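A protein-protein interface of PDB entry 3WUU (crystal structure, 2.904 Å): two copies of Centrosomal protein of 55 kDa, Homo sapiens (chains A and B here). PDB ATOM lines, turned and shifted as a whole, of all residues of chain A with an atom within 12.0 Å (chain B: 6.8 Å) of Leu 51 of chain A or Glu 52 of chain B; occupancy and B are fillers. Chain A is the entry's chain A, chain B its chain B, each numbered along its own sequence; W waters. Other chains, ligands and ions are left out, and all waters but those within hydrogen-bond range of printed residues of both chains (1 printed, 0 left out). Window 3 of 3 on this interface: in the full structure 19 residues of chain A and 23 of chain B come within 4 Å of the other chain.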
ATOM      1  N   TYR A  40     -36.055  13.034 -30.889  1.00  0.00           N
ATOM      2  CA  TYR A  40     -35.696  13.871 -29.750  1.00  0.00           C
ATOM      3  C   TYR A  40     -34.242  14.329 -29.822  1.00  0.00           C
ATOM      4  O   TYR A  40     -33.941  15.499 -29.597  1.00  0.00           O
ATOM      5  CB  TYR A  40     -35.948  13.112 -28.445  1.00  0.00           C
ATOM      6  CG  TYR A  40     -35.777  13.945 -27.198  1.00  0.00           C
ATOM      7  CD1 TYR A  40     -36.683  14.950 -26.881  1.00  0.00           C
ATOM      8  CD2 TYR A  40     -34.721  13.717 -26.327  1.00  0.00           C
ATOM      9  CE1 TYR A  40     -36.537  15.712 -25.736  1.00  0.00           C
ATOM     10  CE2 TYR A  40     -34.566  14.472 -25.178  1.00  0.00           C
ATOM     11  CZ  TYR A  40     -35.475  15.471 -24.887  1.00  0.00           C
ATOM     12  OH  TYR A  40     -35.321  16.224 -23.744  1.00  0.00           O
ATOM     13  N   VAL A  41     -33.345  13.400 -30.141  1.00  0.00           N
ATOM     14  CA  VAL A  41     -31.924  13.707 -30.249  1.00  0.00           C
ATOM     15  C   VAL A  41     -31.647  14.752 -31.329  1.00  0.00           C
ATOM     16  O   VAL A  41     -30.925  15.726 -31.092  1.00  0.00           O
ATOM     17  CB  VAL A  41     -31.096  12.442 -30.519  1.00  0.00           C
ATOM     18  CG1 VAL A  41     -29.663  12.809 -30.874  1.00  0.00           C
ATOM     19  CG2 VAL A  41     -31.129  11.529 -29.306  1.00  0.00           C
ATOM     20  N   LYS A  42     -32.231  14.556 -32.506  1.00  0.00           N
ATOM     21  CA  LYS A  42     -32.084  15.517 -33.590  1.00  0.00           C
ATOM     22  C   LYS A  42     -32.607  16.892 -33.182  1.00  0.00           C
ATOM     23  O   LYS A  42     -32.091  17.918 -33.628  1.00  0.00           O
ATOM     24  CB  LYS A  42     -32.789  15.022 -34.856  1.00  0.00           C
ATOM     25  CG  LYS A  42     -32.089  13.857 -35.550  1.00  0.00           C
ATOM     26  CD  LYS A  42     -32.825  13.465 -36.825  1.00  0.00           C
ATOM     27  CE  LYS A  42     -32.163  12.288 -37.533  1.00  0.00           C
ATOM     28  NZ  LYS A  42     -32.380  10.994 -36.827  1.00  0.00           N
ATOM     29  N   GLY A  43     -33.624  16.907 -32.325  1.00  0.00           N
ATOM     30  CA  GLY A  43     -34.154  18.148 -31.789  1.00  0.00           C
ATOM     31  C   GLY A  43     -33.162  18.827 -30.862  1.00  0.00           C
ATOM     32  O   GLY A  43     -32.909  20.024 -30.980  1.00  0.00           O
ATOM     33  N   LEU A  44     -32.596  18.058 -29.938  1.00  0.00           N
ATOM     34  CA  LEU A  44     -31.612  18.583 -29.000  1.00  0.00           C
ATOM     35  C   LEU A  44     -30.383  19.117 -29.721  1.00  0.00           C
ATOM     36  O   LEU A  44     -29.864  20.176 -29.368  1.00  0.00           O
ATOM     37  CB  LEU A  44     -31.188  17.507 -28.003  1.00  0.00           C
ATOM     38  CG  LEU A  44     -32.226  17.057 -26.980  1.00  0.00           C
ATOM     39  CD1 LEU A  44     -31.552  16.199 -25.925  1.00  0.00           C
ATOM     40  CD2 LEU A  44     -32.910  18.253 -26.349  1.00  0.00           C
ATOM     41  N   LEU A  45     -29.915  18.374 -30.722  1.00  0.00           N
ATOM     42  CA  LEU A  45     -28.757  18.795 -31.506  1.00  0.00           C
ATOM     43  C   LEU A  45     -29.005  20.128 -32.215  1.00  0.00           C
ATOM     44  O   LEU A  45     -28.138  21.005 -32.218  1.00  0.00           O
ATOM     45  CB  LEU A  45     -28.355  17.715 -32.511  1.00  0.00           C
ATOM     46  CG  LEU A  45     -27.700  16.463 -31.921  1.00  0.00           C
ATOM     47  CD1 LEU A  45     -27.386  15.449 -33.009  1.00  0.00           C
ATOM     48  CD2 LEU A  45     -26.445  16.824 -31.145  1.00  0.00           C
ATOM     49  N   ALA A  46     -30.187  20.282 -32.806  1.00  0.00           N
ATOM     50  CA  ALA A  46     -30.564  21.546 -33.433  1.00  0.00           C
ATOM     51  C   ALA A  46     -30.643  22.654 -32.385  1.00  0.00           C
ATOM     52  O   ALA A  46     -30.320  23.809 -32.658  1.00  0.00           O
ATOM     53  CB  ALA A  46     -31.891  21.406 -34.161  1.00  0.00           C
ATOM     54  N   LYS A  47     -31.067  22.283 -31.181  1.00  0.00           N
ATOM     55  CA  LYS A  47     -31.175  23.221 -30.073  1.00  0.00           C
ATOM     56  C   LYS A  47     -29.796  23.653 -29.572  1.00  0.00           C
ATOM     57  O   LYS A  47     -29.571  24.830 -29.305  1.00  0.00           O
ATOM     58  CB  LYS A  47     -31.985  22.590 -28.940  1.00  0.00           C
ATOM     59  CG  LYS A  47     -32.256  23.507 -27.767  1.00  0.00           C
ATOM     60  CD  LYS A  47     -33.247  22.869 -26.806  1.00  0.00           C
ATOM     61  CE  LYS A  47     -33.652  23.831 -25.703  1.00  0.00           C
ATOM     62  NZ  LYS A  47     -34.670  23.229 -24.806  1.00  0.00           N
ATOM     63  N   ILE A  48     -28.877  22.699 -29.445  1.00  0.00           N
ATOM     64  CA  ILE A  48     -27.506  23.003 -29.047  1.00  0.00           C
ATOM     65  C   ILE A  48     -26.856  23.902 -30.089  1.00  0.00           C
ATOM     66  O   ILE A  48     -26.097  24.813 -29.763  1.00  0.00           O
ATOM     67  CB  ILE A  48     -26.662  21.721 -28.916  1.00  0.00           C
ATOM     68  CG1 ILE A  48     -27.203  20.827 -27.803  1.00  0.00           C
ATOM     69  CG2 ILE A  48     -25.210  22.059 -28.636  1.00  0.00           C
ATOM     70  CD1 ILE A  48     -26.421  19.544 -27.627  1.00  0.00           C
ATOM     71  N   PHE A  49     -27.177  23.639 -31.349  1.00  0.00           N
ATOM     72  CA  PHE A  49     -26.609  24.387 -32.462  1.00  0.00           C
ATOM     73  C   PHE A  49     -27.082  25.837 -32.486  1.00  0.00           C
ATOM     74  O   PHE A  49     -26.412  26.699 -33.051  1.00  0.00           O
ATOM     75  CB  PHE A  49     -26.946  23.686 -33.780  1.00  0.00           C
ATOM     76  CG  PHE A  49     -26.326  24.326 -34.990  1.00  0.00           C
ATOM     77  CD1 PHE A  49     -25.020  24.034 -35.350  1.00  0.00           C
ATOM     78  CD2 PHE A  49     -27.057  25.205 -35.780  1.00  0.00           C
ATOM     79  CE1 PHE A  49     -24.446  24.614 -36.468  1.00  0.00           C
ATOM     80  CE2 PHE A  49     -26.492  25.790 -36.898  1.00  0.00           C
ATOM     81  CZ  PHE A  49     -25.185  25.493 -37.243  1.00  0.00           C
ATOM     82  N   GLU A  50     -28.234  26.109 -31.880  1.00  0.00           N
ATOM     83  CA  GLU A  50     -28.737  27.479 -31.790  1.00  0.00           C
ATOM     84  C   GLU A  50     -28.148  28.208 -30.586  1.00  0.00           C
ATOM     85  O   GLU A  50     -27.909  29.416 -30.633  1.00  0.00           O
ATOM     86  CB  GLU A  50     -30.264  27.496 -31.718  1.00  0.00           C
ATOM     87  CG  GLU A  50     -30.936  26.983 -32.976  1.00  0.00           C
ATOM     88  CD  GLU A  50     -30.512  27.758 -34.203  1.00  0.00           C
ATOM     89  OE1 GLU A  50     -30.191  27.122 -35.227  1.00  0.00           O
ATOM     90  OE2 GLU A  50     -30.497  29.005 -34.139  1.00  0.00           O
ATOM     91  N   LEU A  51     -27.912  27.465 -29.509  1.00  0.00           N
ATOM     92  CA  LEU A  51     -27.261  28.001 -28.319  1.00  0.00           C
ATOM     93  C   LEU A  51     -25.781  28.294 -28.572  1.00  0.00           C
ATOM     94  O   LEU A  51     -25.141  28.999 -27.793  1.00  0.00           O
ATOM     95  CB  LEU A  51     -27.404  27.018 -27.157  1.00  0.00           C
ATOM     96  CG  LEU A  51     -28.806  26.862 -26.573  1.00  0.00           C
ATOM     97  CD1 LEU A  51     -28.851  25.678 -25.624  1.00  0.00           C
ATOM     98  CD2 LEU A  51     -29.227  28.134 -25.860  1.00  0.00           C
ATOM     99  N   GLU A  52     -25.237  27.746 -29.655  1.00  0.00           N
ATOM    100  CA  GLU A  52     -23.840  27.975 -29.999  1.00  0.00           C
ATOM    101  C   GLU A  52     -23.679  29.176 -30.925  1.00  0.00           C
ATOM    102  O   GLU A  52     -22.599  29.753 -31.026  1.00  0.00           O
ATOM    103  CB  GLU A  52     -23.213  26.713 -30.601  1.00  0.00           C
ATOM    104  CG  GLU A  52     -22.952  25.600 -29.596  1.00  0.00           C
ATOM    105  CD  GLU A  52     -22.415  24.328 -30.236  1.00  0.00           C
ATOM    106  OE1 GLU A  52     -22.692  24.094 -31.431  1.00  0.00           O
ATOM    107  OE2 GLU A  52     -21.714  23.564 -29.537  1.00  0.00           O
ATOM    108  N   LYS A  53     -24.759  29.546 -31.603  1.00  0.00           N
ATOM    109  CA  LYS A  53     -24.777  30.783 -32.375  1.00  0.00           C
ATOM    110  C   LYS A  53     -24.781  31.978 -31.417  1.00  0.00           C
ATOM    111  O   LYS A  53     -24.299  33.062 -31.749  1.00  0.00           O
ATOM    112  CB  LYS A  53     -25.989  30.827 -33.312  1.00  0.00           C
ATOM    113  CG  LYS A  53     -25.938  29.787 -34.433  1.00  0.00           C
ATOM    114  CD  LYS A  53     -27.251  29.726 -35.211  1.00  0.00           C
ATOM    115  CE  LYS A  53     -27.612  31.076 -35.811  1.00  0.00           C
ATOM    116  NZ  LYS A  53     -28.840  31.011 -36.658  1.00  0.00           N
ATOM    117  N   LYS A  54     -25.315  31.762 -30.217  1.00  0.00           N
ATOM    118  CA  LYS A  54     -25.281  32.768 -29.162  1.00  0.00           C
ATOM    119  C   LYS A  54     -24.000  32.630 -28.341  1.00  0.00           C
ATOM    120  O   LYS A  54     -24.045  32.529 -27.112  1.00  0.00           O
ATOM    121  CB  LYS A  54     -26.516  32.641 -28.266  1.00  0.00           C
ATOM    122  CG  LYS A  54     -27.828  32.924 -28.977  1.00  0.00           C
ATOM    123  CD  LYS A  54     -28.987  32.921 -27.998  1.00  0.00           C
ATOM    124  CE  LYS A  54     -30.231  33.515 -28.635  1.00  0.00           C
ATOM    125  NZ  LYS A  54     -31.400  33.486 -27.711  1.00  0.00           N
ATOM    126  N   THR A  55     -22.863  32.624 -29.034  1.00  0.00           N
ATOM    127  CA  THR A  55     -21.560  32.468 -28.390  1.00  0.00           C
ATOM    128  C   THR A  55     -20.432  32.982 -29.290  1.00  0.00           C
ATOM    129  O   THR A  55     -20.615  33.175 -30.495  1.00  0.00           O
ATOM    130  CB  THR A  55     -21.285  30.989 -28.000  1.00  0.00           C
ATOM    131  OG1 THR A  55     -20.865  30.919 -26.632  1.00  0.00           O
ATOM    132  CG2 THR A  55     -20.202  30.378 -28.888  1.00  0.00           C
ATOM    133  N   LYS B  47     -25.168  19.581 -21.632  1.00  0.00           N
ATOM    134  CA  LYS B  47     -24.480  20.571 -22.442  1.00  0.00           C
ATOM    135  C   LYS B  47     -25.393  21.756 -22.744  1.00  0.00           C
ATOM    136  O   LYS B  47     -24.948  22.902 -22.771  1.00  0.00           O
ATOM    137  CB  LYS B  47     -23.996  19.929 -23.737  1.00  0.00           C
ATOM    138  CG  LYS B  47     -23.220  20.848 -24.652  1.00  0.00           C
ATOM    139  CD  LYS B  47     -22.821  20.100 -25.907  1.00  0.00           C
ATOM    140  CE  LYS B  47     -22.164  21.008 -26.924  1.00  0.00           C
ATOM    141  NZ  LYS B  47     -21.950  20.290 -28.210  1.00  0.00           N
ATOM    142  N   ILE B  48     -26.672  21.471 -22.973  1.00  0.00           N
ATOM    143  CA  ILE B  48     -27.677  22.517 -23.136  1.00  0.00           C
ATOM    144  C   ILE B  48     -27.742  23.371 -21.873  1.00  0.00           C
ATOM    145  O   ILE B  48     -27.847  24.595 -21.940  1.00  0.00           O
ATOM    146  CB  ILE B  48     -29.069  21.919 -23.450  1.00  0.00           C
ATOM    147  CG1 ILE B  48     -29.063  21.268 -24.833  1.00  0.00           C
ATOM    148  CG2 ILE B  48     -30.150  22.987 -23.397  1.00  0.00           C
ATOM    149  CD1 ILE B  48     -30.363  20.605 -25.206  1.00  0.00           C
ATOM    150  N   PHE B  49     -27.656  22.709 -20.722  1.00  0.00           N
ATOM    151  CA  PHE B  49     -27.666  23.377 -19.424  1.00  0.00           C
ATOM    152  C   PHE B  49     -26.509  24.367 -19.289  1.00  0.00           C
ATOM    153  O   PHE B  49     -26.695  25.494 -18.832  1.00  0.00           O
ATOM    154  CB  PHE B  49     -27.595  22.337 -18.303  1.00  0.00           C
ATOM    155  CG  PHE B  49     -27.746  22.915 -16.925  1.00  0.00           C
ATOM    156  CD1 PHE B  49     -29.004  23.100 -16.375  1.00  0.00           C
ATOM    157  CD2 PHE B  49     -26.634  23.262 -16.175  1.00  0.00           C
ATOM    158  CE1 PHE B  49     -29.150  23.626 -15.107  1.00  0.00           C
ATOM    159  CE2 PHE B  49     -26.773  23.792 -14.905  1.00  0.00           C
ATOM    160  CZ  PHE B  49     -28.032  23.973 -14.371  1.00  0.00           C
ATOM    161  N   GLU B  50     -25.318  23.933 -19.689  1.00  0.00           N
ATOM    162  CA  GLU B  50     -24.121  24.759 -19.581  1.00  0.00           C
ATOM    163  C   GLU B  50     -24.142  25.922 -20.568  1.00  0.00           C
ATOM    164  O   GLU B  50     -23.650  27.008 -20.266  1.00  0.00           O
ATOM    165  CB  GLU B  50     -22.869  23.906 -19.793  1.00  0.00           C
ATOM    166  CG  GLU B  50     -22.623  22.878 -18.697  1.00  0.00           C
ATOM    167  CD  GLU B  50     -21.823  23.436 -17.533  1.00  0.00           C
ATOM    168  OE1 GLU B  50     -20.860  24.195 -17.781  1.00  0.00           O
ATOM    169  OE2 GLU B  50     -22.155  23.117 -16.372  1.00  0.00           O
ATOM    170  N   LEU B  51     -24.715  25.692 -21.745  1.00  0.00           N
ATOM    171  CA  LEU B  51     -24.803  26.730 -22.766  1.00  0.00           C
ATOM    172  C   LEU B  51     -25.829  27.800 -22.402  1.00  0.00           C
ATOM    173  O   LEU B  51     -25.684  28.966 -22.773  1.00  0.00           O
ATOM    174  CB  LEU B  51     -25.140  26.119 -24.128  1.00  0.00           C
ATOM    175  CG  LEU B  51     -24.006  25.380 -24.843  1.00  0.00           C
ATOM    176  CD1 LEU B  51     -24.517  24.682 -26.093  1.00  0.00           C
ATOM    177  CD2 LEU B  51     -22.882  26.343 -25.192  1.00  0.00           C
ATOM    178  N   GLU B  52     -26.862  27.402 -21.669  1.00  0.00           N
ATOM    179  CA  GLU B  52     -27.929  28.325 -21.306  1.00  0.00           C
ATOM    180  C   GLU B  52     -27.535  29.261 -20.172  1.00  0.00           C
ATOM    181  O   GLU B  52     -28.136  30.323 -20.001  1.00  0.00           O
ATOM    182  CB  GLU B  52     -29.203  27.564 -20.944  1.00  0.00           C
ATOM    183  CG  GLU B  52     -29.928  26.993 -22.146  1.00  0.00           C
ATOM    184  CD  GLU B  52     -31.218  26.303 -21.767  1.00  0.00           C
ATOM    185  OE1 GLU B  52     -31.410  26.023 -20.564  1.00  0.00           O
ATOM    186  OE2 GLU B  52     -32.041  26.045 -22.671  1.00  0.00           O
ATOM    187  N   LYS B  53     -26.522  28.873 -19.402  1.00  0.00           N
ATOM    188  CA  LYS B  53     -26.033  29.714 -18.311  1.00  0.00           C
ATOM    189  C   LYS B  53     -25.260  30.926 -18.846  1.00  0.00           C
ATOM    190  O   LYS B  53     -24.912  31.833 -18.089  1.00  0.00           O
ATOM    191  CB  LYS B  53     -25.160  28.906 -17.349  1.00  0.00           C
ATOM    192  CG  LYS B  53     -25.885  27.752 -16.669  1.00  0.00           C
ATOM    193  CD  LYS B  53     -24.905  26.653 -16.281  1.00  0.00           C
ATOM    194  CE  LYS B  53     -23.892  27.130 -15.252  1.00  0.00           C
ATOM    195  NZ  LYS B  53     -24.459  27.107 -13.878  1.00  0.00           N
ATOM    196  N   LYS B  54     -25.006  30.935 -20.153  1.00  0.00           N
ATOM    197  CA  LYS B  54     -24.360  32.060 -20.819  1.00  0.00           C
ATOM    198  C   LYS B  54     -25.391  32.982 -21.477  1.00  0.00           C
ATOM    199  O   LYS B  54     -26.153  32.568 -22.350  1.00  0.00           O
ATOM    200  CB  LYS B  54     -23.349  31.557 -21.852  1.00  0.00           C
ATOM    201  CG  LYS B  54     -22.394  30.487 -21.327  1.00  0.00           C
ATOM    202  CD  LYS B  54     -21.432  29.967 -22.403  1.00  0.00           C
ATOM    203  CE  LYS B  54     -20.465  28.918 -21.842  1.00  0.00           C
ATOM    204  NZ  LYS B  54     -19.386  28.513 -22.793  1.00  0.00           N
HETATM  205  O   HOH W   1     -34.193  24.671 -22.494  1.00  0.00           O
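Hydrophobic or aromatic side chains of chain B within 4 Å of the printed part of chain A: Ile 48 and Leu 51.
Along chain B the printed residues that touch a printed residue of chain A span positions 47 to 52.
Hydrophobic or aromatic side chains of chain A within 4 Å of the printed part of chain B: Leu 44, Ile 48 and Leu 51.
Along chain A the printed residues that touch a printed residue of chain B span positions 44 to 52.
Among the printed residues, Asp or Glu carboxylates within 4 Å of a Lys or Arg side-chain nitrogen of the other chain: Glu 52 of chain A with Lys 47 of chain B (3.5 Å).
Gly 43 of chain A touches none of the printed residues of chain B.
Printed residues of chain B within 4 Å of Ile 48 of chain A: Lys 47, Ile 48 and Leu 51.
Of chain B, only Ile 48, Leu 51 and Glu 52 come within 4 Å of Leu 51 of chain A.
Of the printed residues of chain B, Glu 52 of chain A touches Lys 47 and Leu 51.
Printed residues of chain A within 4 Å of Lys 47 of chain B: Ile 48 (3.6 Å) and Glu 52 (3.5 Å).
Of the printed residues of chain A, Ile 48 of chain B touches Leu 44, Ile 48 and Leu 51.
Glu 50 of chain B touches none of the printed residues of chain A.
Of the printed residues of chain A, Leu 51 of chain B touches Ile 48, Leu 51 and Glu 52.
Of chain A, only Leu 51 comes within 4 Å of Glu 52 of chain B.
Lys 53 of chain B touches none of the printed residues of chain A.
No residue of chain A comes within 4 Å of Lys 54 of chain B.
Ile 48 of chain B touches its own counterpart, Ile 48 of chain A.
Leu 51 of chain B touches its own counterpart, Leu 51 of chain A.
Leu 51 of chain A touches Glu 52 of chain B, and with the chains exchanged Glu 52 of chain A touches Leu 51 of chain B.
Glu 52 of chain A touches Lys 47 of chain B, but with the chains exchanged Lys 47 of chain A does not touch Glu 52 of chain B (4.1 Å).
8 positions are printed for both chains.
Among the printed residues, merely in contact across the chains: Ile 48 of chain A with Ile 48 of chain B (3.5 Å), Ile 48 of chain A with Lys 47 of chain B (3.6 Å), Leu 44 of chain A with Ile 48 of chain B (3.7 Å), Ile 48 of chain A with Leu 51 of chain B (3.7 Å), Leu 51 of chain A with Ile 48 of chain B (3.7 Å), Leu 51 of chain A with Leu 51 of chain B (3.9 Å), Leu 51 of chain A with Glu 52 of chain B (3.9 Å) and Glu 52 of chain A with Leu 51 of chain B (3.9 Å).
Water W1 lies within hydrogen-bond range of OE2 of Glu 52 of chain B and NZ of Lys 47 of chain A.
The side-chain carboxylate (OE2) of Glu 52 of chain A is in salt-bridge range of the side-chain amino group (NZ) of Lys 47 of chain B, at 3.5 Å.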
